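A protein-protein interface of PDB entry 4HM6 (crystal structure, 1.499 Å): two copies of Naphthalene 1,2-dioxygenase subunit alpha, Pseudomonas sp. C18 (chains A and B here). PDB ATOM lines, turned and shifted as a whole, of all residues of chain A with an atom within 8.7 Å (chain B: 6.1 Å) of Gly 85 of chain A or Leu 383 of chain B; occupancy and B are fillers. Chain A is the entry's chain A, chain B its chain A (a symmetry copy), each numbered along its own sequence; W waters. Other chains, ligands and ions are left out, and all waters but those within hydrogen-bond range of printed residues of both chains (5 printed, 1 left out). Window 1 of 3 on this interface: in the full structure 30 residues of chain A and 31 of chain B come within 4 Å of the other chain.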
ATOM      1  N   ASN A  79      15.284 -22.300  22.673  1.00  0.00           N
ATOM      2  CA  ASN A  79      14.666 -21.856  21.430  1.00  0.00           C
ATOM      3  C   ASN A  79      15.727 -21.719  20.335  1.00  0.00           C
ATOM      4  O   ASN A  79      15.932 -20.641  19.755  1.00  0.00           O
ATOM      5  CB  ASN A  79      13.942 -20.532  21.679  1.00  0.00           C
ATOM      6  CG  ASN A  79      13.071 -20.117  20.524  1.00  0.00           C
ATOM      7  OD1 ASN A  79      12.831 -20.890  19.583  1.00  0.00           O
ATOM      8  ND2 ASN A  79      12.592 -18.882  20.578  1.00  0.00           N
ATOM      9  N   VAL A  80      16.419 -22.821  20.072  1.00  0.00           N
ATOM     10  CA  VAL A  80      17.573 -22.819  19.183  1.00  0.00           C
ATOM     11  C   VAL A  80      17.577 -24.111  18.379  1.00  0.00           C
ATOM     12  O   VAL A  80      17.552 -25.209  18.950  1.00  0.00           O
ATOM     13  CB  VAL A  80      18.905 -22.713  19.972  1.00  0.00           C
ATOM     14  CG1 VAL A  80      20.095 -22.736  19.012  1.00  0.00           C
ATOM     15  CG2 VAL A  80      18.944 -21.464  20.861  1.00  0.00           C
ATOM     16  N   CYS A  81      17.595 -23.992  17.054  1.00  0.00           N
ATOM     17  CA  CYS A  81      17.593 -25.173  16.193  1.00  0.00           C
ATOM     18  C   CYS A  81      18.881 -25.992  16.329  1.00  0.00           C
ATOM     19  O   CYS A  81      19.976 -25.427  16.422  1.00  0.00           O
ATOM     20  CB  CYS A  81      17.405 -24.760  14.732  1.00  0.00           C
ATOM     21  SG  CYS A  81      17.265 -26.148  13.617  1.00  0.00           S
ATOM     22  N   ARG A  82      18.746 -27.317  16.332  1.00  0.00           N
ATOM     23  CA  ARG A  82      19.887 -28.221  16.533  1.00  0.00           C
ATOM     24  C   ARG A  82      20.763 -28.375  15.294  1.00  0.00           C
ATOM     25  O   ARG A  82      21.800 -29.038  15.342  1.00  0.00           O
ATOM     26  CB  ARG A  82      19.419 -29.615  16.985  1.00  0.00           C
ATOM     27  CG  ARG A  82      18.883 -29.709  18.417  1.00  0.00           C
ATOM     28  CD  ARG A  82      19.960 -29.448  19.479  1.00  0.00           C
ATOM     29  NE  ARG A  82      21.212 -30.165  19.238  1.00  0.00           N
ATOM     30  CZ  ARG A  82      21.460 -31.416  19.622  1.00  0.00           C
ATOM     31  NH1 ARG A  82      20.531 -32.122  20.268  1.00  0.00           N
ATOM     32  NH2 ARG A  82      22.639 -31.971  19.349  1.00  0.00           N
ATOM     33  N   HIS A  83      20.339 -27.784  14.182  1.00  0.00           N
ATOM     34  CA  HIS A  83      21.102 -27.858  12.936  1.00  0.00           C
ATOM     35  C   HIS A  83      22.161 -26.751  12.894  1.00  0.00           C
ATOM     36  O   HIS A  83      23.299 -26.971  13.318  1.00  0.00           O
ATOM     37  CB  HIS A  83      20.169 -27.801  11.723  1.00  0.00           C
ATOM     38  CG  HIS A  83      20.876 -27.884  10.401  1.00  0.00           C
ATOM     39  ND1 HIS A  83      20.510 -27.119   9.312  1.00  0.00           N
ATOM     40  CD2 HIS A  83      21.914 -28.649   9.986  1.00  0.00           C
ATOM     41  CE1 HIS A  83      21.295 -27.401   8.285  1.00  0.00           C
ATOM     42  NE2 HIS A  83      22.158 -28.325   8.670  1.00  0.00           N
ATOM     43  N   ARG A  84      21.794 -25.561  12.412  1.00  0.00           N
ATOM     44  CA  ARG A  84      22.733 -24.435  12.367  1.00  0.00           C
ATOM     45  C   ARG A  84      22.379 -23.303  13.343  1.00  0.00           C
ATOM     46  O   ARG A  84      22.832 -22.172  13.154  1.00  0.00           O
ATOM     47  CB  ARG A  84      22.858 -23.834  10.952  1.00  0.00           C
ATOM     48  CG  ARG A  84      23.184 -24.785   9.798  1.00  0.00           C
ATOM     49  CD  ARG A  84      24.599 -25.364   9.832  1.00  0.00           C
ATOM     50  NE  ARG A  84      25.681 -24.385  10.009  1.00  0.00           N
ATOM     51  CZ  ARG A  84      26.897 -24.728  10.438  1.00  0.00           C
ATOM     52  NH1 ARG A  84      27.155 -26.003  10.702  1.00  0.00           N
ATOM     53  NH2 ARG A  84      27.854 -23.821  10.612  1.00  0.00           N
ATOM     54  N   GLY A  85      21.545 -23.582  14.349  1.00  0.00           N
ATOM     55  CA  GLY A  85      21.413 -22.688  15.492  1.00  0.00           C
ATOM     56  C   GLY A  85      20.516 -21.473  15.361  1.00  0.00           C
ATOM     57  O   GLY A  85      20.613 -20.540  16.164  1.00  0.00           O
ATOM     58  N   LYS A  86      19.631 -21.485  14.366  1.00  0.00           N
ATOM     59  CA  LYS A  86      18.684 -20.392  14.164  1.00  0.00           C
ATOM     60  C   LYS A  86      17.646 -20.385  15.286  1.00  0.00           C
ATOM     61  O   LYS A  86      17.344 -21.431  15.859  1.00  0.00           O
ATOM     62  CB  LYS A  86      17.983 -20.573  12.815  1.00  0.00           C
ATOM     63  CG  LYS A  86      17.350 -19.318  12.297  1.00  0.00           C
ATOM     64  CD  LYS A  86      15.876 -19.510  12.115  1.00  0.00           C
ATOM     65  CE  LYS A  86      15.195 -18.170  11.986  1.00  0.00           C
ATOM     66  NZ  LYS A  86      13.802 -18.243  12.478  1.00  0.00           N
ATOM     67  N   THR A  87      17.110 -19.215  15.620  1.00  0.00           N
ATOM     68  CA  THR A  87      16.036 -19.155  16.613  1.00  0.00           C
ATOM     69  C   THR A  87      14.779 -19.811  16.045  1.00  0.00           C
ATOM     70  O   THR A  87      14.294 -19.442  14.977  1.00  0.00           O
ATOM     71  CB  THR A  87      15.747 -17.709  17.057  1.00  0.00           C
ATOM     72  OG1 THR A  87      16.883 -17.209  17.773  1.00  0.00           O
ATOM     73  CG2 THR A  87      14.522 -17.641  17.979  1.00  0.00           C
ATOM     74  N   LEU A  88      14.250 -20.791  16.760  1.00  0.00           N
ATOM     75  CA  LEU A  88      13.175 -21.625  16.223  1.00  0.00           C
ATOM     76  C   LEU A  88      11.823 -20.889  16.177  1.00  0.00           C
ATOM     77  O   LEU A  88      11.150 -20.851  15.132  1.00  0.00           O
ATOM     78  CB  LEU A  88      13.084 -22.905  17.053  1.00  0.00           C
ATOM     79  CG  LEU A  88      12.304 -24.094  16.516  1.00  0.00           C
ATOM     80  CD1 LEU A  88      12.810 -24.512  15.130  1.00  0.00           C
ATOM     81  CD2 LEU A  88      12.395 -25.254  17.518  1.00  0.00           C
ATOM     82  N   CYS A 101      11.781 -25.022  11.698  1.00  0.00           N
ATOM     83  CA  CYS A 101      12.787 -23.986  11.523  1.00  0.00           C
ATOM     84  C   CYS A 101      12.715 -23.348  10.139  1.00  0.00           C
ATOM     85  O   CYS A 101      12.646 -24.052   9.133  1.00  0.00           O
ATOM     86  CB  CYS A 101      14.166 -24.590  11.715  1.00  0.00           C
ATOM     87  SG  CYS A 101      15.489 -23.395  11.633  1.00  0.00           S
ATOM     88  N   TYR A 103      14.980 -21.893   8.462  1.00  0.00           N
ATOM     89  CA  TYR A 103      16.230 -21.911   7.717  1.00  0.00           C
ATOM     90  C   TYR A 103      16.241 -23.111   6.756  1.00  0.00           C
ATOM     91  O   TYR A 103      16.126 -22.933   5.532  1.00  0.00           O
ATOM     92  CB  TYR A 103      17.420 -21.890   8.683  1.00  0.00           C
ATOM     93  CG  TYR A 103      18.743 -21.418   8.088  1.00  0.00           C
ATOM     94  CD1 TYR A 103      18.929 -21.320   6.711  1.00  0.00           C
ATOM     95  CD2 TYR A 103      19.804 -21.084   8.909  1.00  0.00           C
ATOM     96  CE1 TYR A 103      20.137 -20.896   6.176  1.00  0.00           C
ATOM     97  CE2 TYR A 103      21.018 -20.665   8.388  1.00  0.00           C
ATOM     98  CZ  TYR A 103      21.178 -20.575   7.019  1.00  0.00           C
ATOM     99  OH  TYR A 103      22.387 -20.159   6.501  1.00  0.00           O
ATOM    100  N   HIS A 104      16.345 -24.328   7.289  1.00  0.00           N
ATOM    101  CA  HIS A 104      16.307 -25.515   6.429  1.00  0.00           C
ATOM    102  C   HIS A 104      15.099 -26.428   6.674  1.00  0.00           C
ATOM    103  O   HIS A 104      15.035 -27.531   6.139  1.00  0.00           O
ATOM    104  CB  HIS A 104      17.618 -26.321   6.507  1.00  0.00           C
ATOM    105  CG  HIS A 104      18.857 -25.482   6.414  1.00  0.00           C
ATOM    106  ND1 HIS A 104      19.398 -24.823   7.497  1.00  0.00           N
ATOM    107  CD2 HIS A 104      19.665 -25.200   5.367  1.00  0.00           C
ATOM    108  CE1 HIS A 104      20.488 -24.177   7.127  1.00  0.00           C
ATOM    109  NE2 HIS A 104      20.669 -24.383   5.836  1.00  0.00           N
ATOM    110  N   TRP A 106      13.803 -28.033   9.364  1.00  0.00           N
ATOM    111  CA  TRP A 106      13.759 -29.119  10.345  1.00  0.00           C
ATOM    112  C   TRP A 106      12.547 -28.951  11.252  1.00  0.00           C
ATOM    113  O   TRP A 106      12.239 -27.835  11.692  1.00  0.00           O
ATOM    114  CB  TRP A 106      15.028 -29.164  11.194  1.00  0.00           C
ATOM    115  CG  TRP A 106      16.226 -29.758  10.508  1.00  0.00           C
ATOM    116  CD1 TRP A 106      16.449 -29.850   9.167  1.00  0.00           C
ATOM    117  CD2 TRP A 106      17.374 -30.336  11.149  1.00  0.00           C
ATOM    118  NE1 TRP A 106      17.670 -30.448   8.933  1.00  0.00           N
ATOM    119  CE2 TRP A 106      18.256 -30.757  10.134  1.00  0.00           C
ATOM    120  CE3 TRP A 106      17.743 -30.532  12.488  1.00  0.00           C
ATOM    121  CZ2 TRP A 106      19.482 -31.369  10.407  1.00  0.00           C
ATOM    122  CZ3 TRP A 106      18.971 -31.146  12.761  1.00  0.00           C
ATOM    123  CH2 TRP A 106      19.822 -31.557  11.721  1.00  0.00           C
ATOM    124  N   PHE A 108      10.543 -29.935  14.719  1.00  0.00           N
ATOM    125  CA  PHE A 108      10.629 -30.472  16.069  1.00  0.00           C
ATOM    126  C   PHE A 108       9.245 -30.587  16.689  1.00  0.00           C
ATOM    127  O   PHE A 108       8.386 -29.728  16.474  1.00  0.00           O
ATOM    128  CB  PHE A 108      11.504 -29.565  16.938  1.00  0.00           C
ATOM    129  CG  PHE A 108      12.917 -29.433  16.448  1.00  0.00           C
ATOM    130  CD1 PHE A 108      13.266 -28.421  15.558  1.00  0.00           C
ATOM    131  CD2 PHE A 108      13.903 -30.313  16.887  1.00  0.00           C
ATOM    132  CE1 PHE A 108      14.579 -28.288  15.098  1.00  0.00           C
ATOM    133  CE2 PHE A 108      15.222 -30.190  16.441  1.00  0.00           C
ATOM    134  CZ  PHE A 108      15.559 -29.180  15.540  1.00  0.00           C
ATOM    135  N   LEU A 133      19.131 -35.616  18.365  1.00  0.00           N
ATOM    136  CA  LEU A 133      19.059 -34.249  17.865  1.00  0.00           C
ATOM    137  C   LEU A 133      17.823 -33.510  18.345  1.00  0.00           C
ATOM    138  O   LEU A 133      17.379 -32.552  17.708  1.00  0.00           O
ATOM    139  CB  LEU A 133      19.125 -34.240  16.338  1.00  0.00           C
ATOM    140  CG  LEU A 133      20.498 -34.622  15.796  1.00  0.00           C
ATOM    141  CD1 LEU A 133      20.499 -34.699  14.286  1.00  0.00           C
ATOM    142  CD2 LEU A 133      21.511 -33.611  16.282  1.00  0.00           C
ATOM    143  N   LEU B  14      33.004 -31.558  10.797  1.00  0.00           N
ATOM    144  CA  LEU B  14      31.647 -32.080  10.952  1.00  0.00           C
ATOM    145  C   LEU B  14      30.748 -31.191  11.806  1.00  0.00           C
ATOM    146  O   LEU B  14      29.521 -31.248  11.697  1.00  0.00           O
ATOM    147  CB  LEU B  14      31.672 -33.499  11.521  1.00  0.00           C
ATOM    148  CG  LEU B  14      32.128 -34.528  10.491  1.00  0.00           C
ATOM    149  CD1 LEU B  14      32.356 -35.886  11.121  1.00  0.00           C
ATOM    150  CD2 LEU B  14      31.081 -34.634   9.406  1.00  0.00           C
ATOM    151  N   SER B  15      31.363 -30.376  12.657  1.00  0.00           N
ATOM    152  CA  SER B  15      30.613 -29.487  13.529  1.00  0.00           C
ATOM    153  C   SER B  15      31.491 -28.333  13.983  1.00  0.00           C
ATOM    154  O   SER B  15      32.720 -28.410  13.896  1.00  0.00           O
ATOM    155  CB  SER B  15      30.059 -30.234  14.745  1.00  0.00           C
ATOM    156  OG  SER B  15      31.104 -30.702  15.586  1.00  0.00           O
ATOM    157  N   GLN B  16      30.854 -27.259  14.449  1.00  0.00           N
ATOM    158  CA  GLN B  16      31.567 -26.097  14.974  1.00  0.00           C
ATOM    159  C   GLN B  16      30.886 -25.644  16.256  1.00  0.00           C
ATOM    160  O   GLN B  16      29.655 -25.727  16.368  1.00  0.00           O
ATOM    161  CB  GLN B  16      31.539 -24.931  13.976  1.00  0.00           C
ATOM    162  CG  GLN B  16      32.015 -25.260  12.553  1.00  0.00           C
ATOM    163  CD  GLN B  16      30.971 -26.005  11.742  1.00  0.00           C
ATOM    164  OE1 GLN B  16      29.797 -25.631  11.737  1.00  0.00           O
ATOM    165  NE2 GLN B  16      31.392 -27.071  11.054  1.00  0.00           N
ATOM    166  N   LYS B  17      31.662 -25.144  17.217  1.00  0.00           N
ATOM    167  CA  LYS B  17      31.059 -24.575  18.423  1.00  0.00           C
ATOM    168  C   LYS B  17      30.286 -23.310  18.072  1.00  0.00           C
ATOM    169  O   LYS B  17      30.785 -22.458  17.334  1.00  0.00           O
ATOM    170  CB  LYS B  17      32.120 -24.264  19.484  1.00  0.00           C
ATOM    171  CG  LYS B  17      32.762 -25.514  20.084  1.00  0.00           C
ATOM    172  CD  LYS B  17      31.686 -26.400  20.738  1.00  0.00           C
ATOM    173  CE  LYS B  17      32.279 -27.634  21.400  1.00  0.00           C
ATOM    174  NZ  LYS B  17      31.206 -28.475  22.024  1.00  0.00           N
ATOM    175  N   HIS B  18      29.068 -23.186  18.600  1.00  0.00           N
ATOM    176  CA  HIS B  18      28.183 -22.074  18.256  1.00  0.00           C
ATOM    177  C   HIS B  18      28.814 -20.741  18.653  1.00  0.00           C
ATOM    178  O   HIS B  18      28.567 -19.719  18.009  1.00  0.00           O
ATOM    179  CB  HIS B  18      26.809 -22.281  18.912  1.00  0.00           C
ATOM    180  CG  HIS B  18      25.681 -21.531  18.260  1.00  0.00           C
ATOM    181  ND1 HIS B  18      24.361 -21.848  18.484  1.00  0.00           N
ATOM    182  CD2 HIS B  18      25.679 -20.480  17.405  1.00  0.00           C
ATOM    183  CE1 HIS B  18      23.587 -21.027  17.790  1.00  0.00           C
ATOM    184  NE2 HIS B  18      24.362 -20.183  17.134  1.00  0.00           N
ATOM    185  N   LEU B  19      29.666 -20.754  19.681  1.00  0.00           N
ATOM    186  CA  LEU B  19      30.348 -19.535  20.122  1.00  0.00           C
ATOM    187  C   LEU B  19      31.144 -18.850  19.010  1.00  0.00           C
ATOM    188  O   LEU B  19      31.407 -17.651  19.090  1.00  0.00           O
ATOM    189  CB  LEU B  19      31.256 -19.807  21.333  1.00  0.00           C
ATOM    190  CG  LEU B  19      32.541 -20.600  21.057  1.00  0.00           C
ATOM    191  CD1 LEU B  19      33.722 -19.703  20.696  1.00  0.00           C
ATOM    192  CD2 LEU B  19      32.896 -21.465  22.254  1.00  0.00           C
ATOM    193  N   ILE B  20      31.528 -19.584  17.966  1.00  0.00           N
ATOM    194  CA  ILE B  20      32.316 -18.941  16.913  1.00  0.00           C
ATOM    195  C   ILE B  20      31.561 -17.776  16.246  1.00  0.00           C
ATOM    196  O   ILE B  20      32.190 -16.857  15.715  1.00  0.00           O
ATOM    197  CB  ILE B  20      32.886 -19.931  15.849  1.00  0.00           C
ATOM    198  CG1 ILE B  20      31.780 -20.484  14.936  1.00  0.00           C
ATOM    199  CG2 ILE B  20      33.735 -21.038  16.509  1.00  0.00           C
ATOM    200  CD1 ILE B  20      32.322 -21.293  13.749  1.00  0.00           C
ATOM    201  N   HIS B  21      30.224 -17.789  16.294  1.00  0.00           N
ATOM    202  CA  HIS B  21      29.448 -16.684  15.718  1.00  0.00           C
ATOM    203  C   HIS B  21      29.218 -15.527  16.680  1.00  0.00           C
ATOM    204  O   HIS B  21      28.655 -14.502  16.287  1.00  0.00           O
ATOM    205  CB  HIS B  21      28.076 -17.168  15.220  1.00  0.00           C
ATOM    206  CG  HIS B  21      28.139 -18.100  14.053  1.00  0.00           C
ATOM    207  ND1 HIS B  21      29.197 -18.117  13.170  1.00  0.00           N
ATOM    208  CD2 HIS B  21      27.267 -19.040  13.621  1.00  0.00           C
ATOM    209  CE1 HIS B  21      28.977 -19.038  12.245  1.00  0.00           C
ATOM    210  NE2 HIS B  21      27.811 -19.612  12.495  1.00  0.00           N
ATOM    211  N   GLU B 200      29.188 -18.838   5.053  1.00  0.00           N
ATOM    212  CA  GLU B 200      28.936 -20.283   5.020  1.00  0.00           C
ATOM    213  C   GLU B 200      27.718 -20.583   4.161  1.00  0.00           C
ATOM    214  O   GLU B 200      27.647 -21.618   3.493  1.00  0.00           O
ATOM    215  CB  GLU B 200      28.763 -20.885   6.440  1.00  0.00           C
ATOM    216  CG  GLU B 200      27.395 -20.613   7.072  1.00  0.00           C
ATOM    217  CD  GLU B 200      27.217 -21.232   8.453  1.00  0.00           C
ATOM    218  OE1 GLU B 200      28.231 -21.457   9.155  1.00  0.00           O
ATOM    219  OE2 GLU B 200      26.050 -21.479   8.838  1.00  0.00           O
ATOM    220  N   THR B 368      19.841 -14.308  13.845  1.00  0.00           N
ATOM    221  CA  THR B 368      19.557 -15.062  15.068  1.00  0.00           C
ATOM    222  C   THR B 368      20.562 -16.185  15.286  1.00  0.00           C
ATOM    223  O   THR B 368      20.948 -16.455  16.415  1.00  0.00           O
ATOM    224  CB  THR B 368      18.109 -15.606  15.154  1.00  0.00           C
ATOM    225  OG1 THR B 368      17.885 -16.585  14.136  1.00  0.00           O
ATOM    226  CG2 THR B 368      17.090 -14.476  15.030  1.00  0.00           C
ATOM    227  N   ALA B 369      20.990 -16.847  14.212  1.00  0.00           N
ATOM    228  CA  ALA B 369      22.006 -17.891  14.365  1.00  0.00           C
ATOM    229  C   ALA B 369      23.287 -17.292  14.942  1.00  0.00           C
ATOM    230  O   ALA B 369      23.965 -17.923  15.751  1.00  0.00           O
ATOM    231  CB  ALA B 369      22.289 -18.580  13.044  1.00  0.00           C
ATOM    232  N   SER B 370      23.613 -16.073  14.529  1.00  0.00           N
ATOM    233  CA  SER B 370      24.808 -15.412  15.032  1.00  0.00           C
ATOM    234  C   SER B 370      24.626 -14.973  16.470  1.00  0.00           C
ATOM    235  O   SER B 370      25.502 -15.176  17.300  1.00  0.00           O
ATOM    236  CB  SER B 370      25.173 -14.199  14.176  1.00  0.00           C
ATOM    237  OG  SER B 370      25.393 -14.565  12.831  1.00  0.00           O
ATOM    238  N   ASN B 372      22.580 -16.049  18.744  1.00  0.00           N
ATOM    239  CA  ASN B 372      22.449 -17.176  19.659  1.00  0.00           C
ATOM    240  C   ASN B 372      23.809 -17.692  20.100  1.00  0.00           C
ATOM    241  O   ASN B 372      23.922 -18.317  21.150  1.00  0.00           O
ATOM    242  CB  ASN B 372      21.614 -18.304  19.031  1.00  0.00           C
ATOM    243  CG  ASN B 372      20.137 -17.982  19.007  1.00  0.00           C
ATOM    244  OD1 ASN B 372      19.662 -17.170  19.804  1.00  0.00           O
ATOM    245  ND2 ASN B 372      19.402 -18.606  18.093  1.00  0.00           N
ATOM    246  N   SER B 381      27.510 -25.375  22.387  1.00  0.00           N
ATOM    247  CA  SER B 381      26.723 -26.303  21.574  1.00  0.00           C
ATOM    248  C   SER B 381      27.336 -26.480  20.193  1.00  0.00           C
ATOM    249  O   SER B 381      28.154 -25.667  19.763  1.00  0.00           O
ATOM    250  CB  SER B 381      25.271 -25.835  21.454  1.00  0.00           C
ATOM    251  OG  SER B 381      24.639 -25.834  22.725  1.00  0.00           O
ATOM    252  N   ASP B 382      26.929 -27.539  19.500  1.00  0.00           N
ATOM    253  CA  ASP B 382      27.524 -27.885  18.216  1.00  0.00           C
ATOM    254  C   ASP B 382      26.617 -27.592  17.023  1.00  0.00           C
ATOM    255  O   ASP B 382      25.532 -28.169  16.894  1.00  0.00           O
ATOM    256  CB  ASP B 382      27.916 -29.364  18.208  1.00  0.00           C
ATOM    257  CG  ASP B 382      28.818 -29.724  19.360  1.00  0.00           C
ATOM    258  OD1 ASP B 382      29.861 -29.062  19.517  1.00  0.00           O
ATOM    259  OD2 ASP B 382      28.477 -30.650  20.122  1.00  0.00           O
ATOM    260  N   LEU B 383      27.067 -26.682  16.162  1.00  0.00           N
ATOM    261  CA  LEU B 383      26.439 -26.461  14.856  1.00  0.00           C
ATOM    262  C   LEU B 383      26.821 -27.621  13.946  1.00  0.00           C
ATOM    263  O   LEU B 383      27.998 -27.973  13.854  1.00  0.00           O
ATOM    264  CB  LEU B 383      26.949 -25.157  14.250  1.00  0.00           C
ATOM    265  CG  LEU B 383      26.771 -23.883  15.068  1.00  0.00           C
ATOM    266  CD1 LEU B 383      27.628 -22.791  14.465  1.00  0.00           C
ATOM    267  CD2 LEU B 383      25.300 -23.462  15.088  1.00  0.00           C
ATOM    268  N   LEU B 384      25.839 -28.218  13.273  1.00  0.00           N
ATOM    269  CA  LEU B 384      26.080 -29.435  12.496  1.00  0.00           C
ATOM    270  C   LEU B 384      26.305 -29.164  11.018  1.00  0.00           C
ATOM    271  O   LEU B 384      25.563 -28.402  10.398  1.00  0.00           O
ATOM    272  CB  LEU B 384      24.905 -30.396  12.641  1.00  0.00           C
ATOM    273  CG  LEU B 384      24.583 -30.828  14.058  1.00  0.00           C
ATOM    274  CD1 LEU B 384      23.421 -31.804  14.010  1.00  0.00           C
ATOM    275  CD2 LEU B 384      25.811 -31.451  14.704  1.00  0.00           C
ATOM    276  N   SER B 385      27.335 -29.792  10.454  1.00  0.00           N
ATOM    277  CA  SER B 385      27.547 -29.740   9.009  1.00  0.00           C
ATOM    278  C   SER B 385      28.000 -31.098   8.487  1.00  0.00           C
ATOM    279  O   SER B 385      29.037 -31.220   7.827  1.00  0.00           O
ATOM    280  CB  SER B 385      28.521 -28.624   8.623  1.00  0.00           C
ATOM    281  OG  SER B 385      29.727 -28.706   9.356  1.00  0.00           O
ATOM    282  N   TYR B 417      35.263 -24.699   7.065  1.00  0.00           N
ATOM    283  CA  TYR B 417      35.587 -24.707   8.486  1.00  0.00           C
ATOM    284  C   TYR B 417      36.870 -25.459   8.812  1.00  0.00           C
ATOM    285  O   TYR B 417      37.529 -25.148   9.808  1.00  0.00           O
ATOM    286  CB  TYR B 417      34.394 -25.152   9.345  1.00  0.00           C
ATOM    287  CG  TYR B 417      33.391 -24.031   9.479  1.00  0.00           C
ATOM    288  CD1 TYR B 417      33.743 -22.840  10.125  1.00  0.00           C
ATOM    289  CD2 TYR B 417      32.113 -24.130   8.926  1.00  0.00           C
ATOM    290  CE1 TYR B 417      32.844 -21.788  10.231  1.00  0.00           C
ATOM    291  CE2 TYR B 417      31.202 -23.075   9.034  1.00  0.00           C
ATOM    292  CZ  TYR B 417      31.577 -21.914   9.689  1.00  0.00           C
ATOM    293  OH  TYR B 417      30.700 -20.856   9.795  1.00  0.00           O
HETATM  294  O   HOH W   1      24.358 -19.231   7.939  1.00  0.00           O
HETATM  295  O   HOH W   2      23.517 -29.852  17.261  1.00  0.00           O
HETATM  296  O   HOH W   3      25.492 -21.203  11.740  1.00  0.00           O
HETATM  297  O   HOH W   4      17.266 -18.339  21.113  1.00  0.00           O
HETATM  298  O   HOH W   5      25.797 -31.558  20.152  1.00  0.00           O
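The side-chain sulfur (SG) of Cys 81 of chain A sits close to the backbone NH (N) of His 83 of chain A (3.5 Å). The backbone NH of Cys 81 of chain A lies within hydrogen-bond range of the backbone carbonyl oxygen of Lys 86 of chain A. N of Ser 385 of chain B is in hydrogen-bond range of O of Leu 14 of chain B. The backbone NH of Leu 383 of chain B is in hydrogen-bond range of the backbone carbonyl oxygen of Gln 16 of chain B (2.8 Å). The side-chain hydroxyl (OG) of Ser 385 of chain B is in hydrogen-bond range of the side-chain amide nitrogen (NE2) of Gln 16 of chain B, 2.9 Å away. The side-chain carboxylate (OE1) of Glu 200 of chain B lies within hydrogen-bond range of the side-chain hydroxyl (OH) of Tyr 417 of chain B (2.6 Å).
Gly 85 of chain A touches four residues of chain B. Of chain A, only His 83, Arg 84 and Gly 85 come within 4 Å of Leu 383 of chain B. Ala 369 of chain B touches two residues of chain A. Printed residues of chain B within 4 Å of Thr 87 of chain A: Thr 368 and Asn 372. Of the printed residues of chain A, Gln 16 of chain B touches Arg 84 (2.9 Å). Lys 17 of chain B touches none of the printed residues of chain A. Ser 381 of chain B touches none of the printed residues of chain A. The nearest printed residue of chain B that does not touch Thr 87 of chain A is Ala 369 of chain B (4.8 Å).
Water W1 lies within hydrogen-bond range of the side-chain hydroxyl of Tyr 103 of chain A and the side-chain carboxylate of Glu 200 of chain B. Water W2 lies within hydrogen-bond range of the backbone carbonyl oxygen of Asp 382 of chain B (2.7 Å) and the backbone carbonyl oxygen of Arg 82 of chain A (2.7 Å). Water W5 lies within hydrogen-bond range of the side-chain carboxylate of Asp 382 of chain B (2.8 Å) and the guanidinium group of Arg 82 of chain A (3.3 Å). Water W4 bridges OD1 of Asn 372 of chain B (3.0 Å) and O of Asn 79 of chain A (3.0 Å).
Printed residues of chain A that touch a printed residue of chain B: Arg 82, His 83, Arg 84, Gly 85, Lys 86, Thr 87 and Leu 133. Hydrophobic or aromatic side chains of chain B that line the printed part of chain A: His 18, Ala 369, Leu 383, Leu 384 and Tyr 417.
Among the printed residues, merely in contact across the chains: Arg 82 of chain A with Leu 384 of chain B, His 83 of chain A with Leu 383 of chain B, Arg 84 of chain A with Ala 369 of chain B, Arg 84 of chain A with Leu 383 of chain B, Arg 84 of chain A with Ser 385 of chain B, Arg 84 of chain A with Tyr 417 of chain B, Gly 85 of chain A with His 18 of chain B, Gly 85 of chain A with Ala 369 of chain B, Gly 85 of chain A with Leu 383 of chain B, Lys 86 of chain A with Thr 368 of chain B, Lys 86 of chain A with Asn 372 of chain B and Leu 133 of chain A with Leu 384 of chain B.
The backbone carbonyl oxygen (O) of His 83 of chain A is in hydrogen-bond range of the backbone NH (N) of Leu 384 of chain B (2.8 Å). The side-chain amide oxygen (OE1) of Gln 16 of chain B is in hydrogen-bond range of the guanidinium group (NH1) of Arg 84 of chain A (2.9 Å). The side-chain carboxylate (OE1) of Glu 200 of chain B is in salt-bridge range of the guanidinium group (NH2) of Arg 84 of chain A, 2.8 Å away. The backbone carbonyl oxygen (O) of Leu 384 of chain B sits at hydrogen-bond distance from the guanidinium group (NH1) of Arg 84 of chain A, 2.9 Å away. O of Gly 85 of chain A is in hydrogen-bond range of ND2 of Asn 372 of chain B (3.0 Å). N of Thr 87 of chain A is in hydrogen-bond range of OG1 of Thr 368 of chain B (3.1 Å). ND2 of Asn 372 of chain B is in hydrogen-bond range of OG1 of Thr 87 of chain A (2.9 Å).
No position is printed for both chains. Of the 19 pairs that touch across the chains among the printed residues, none has its exchanged pair printed and touching as well.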
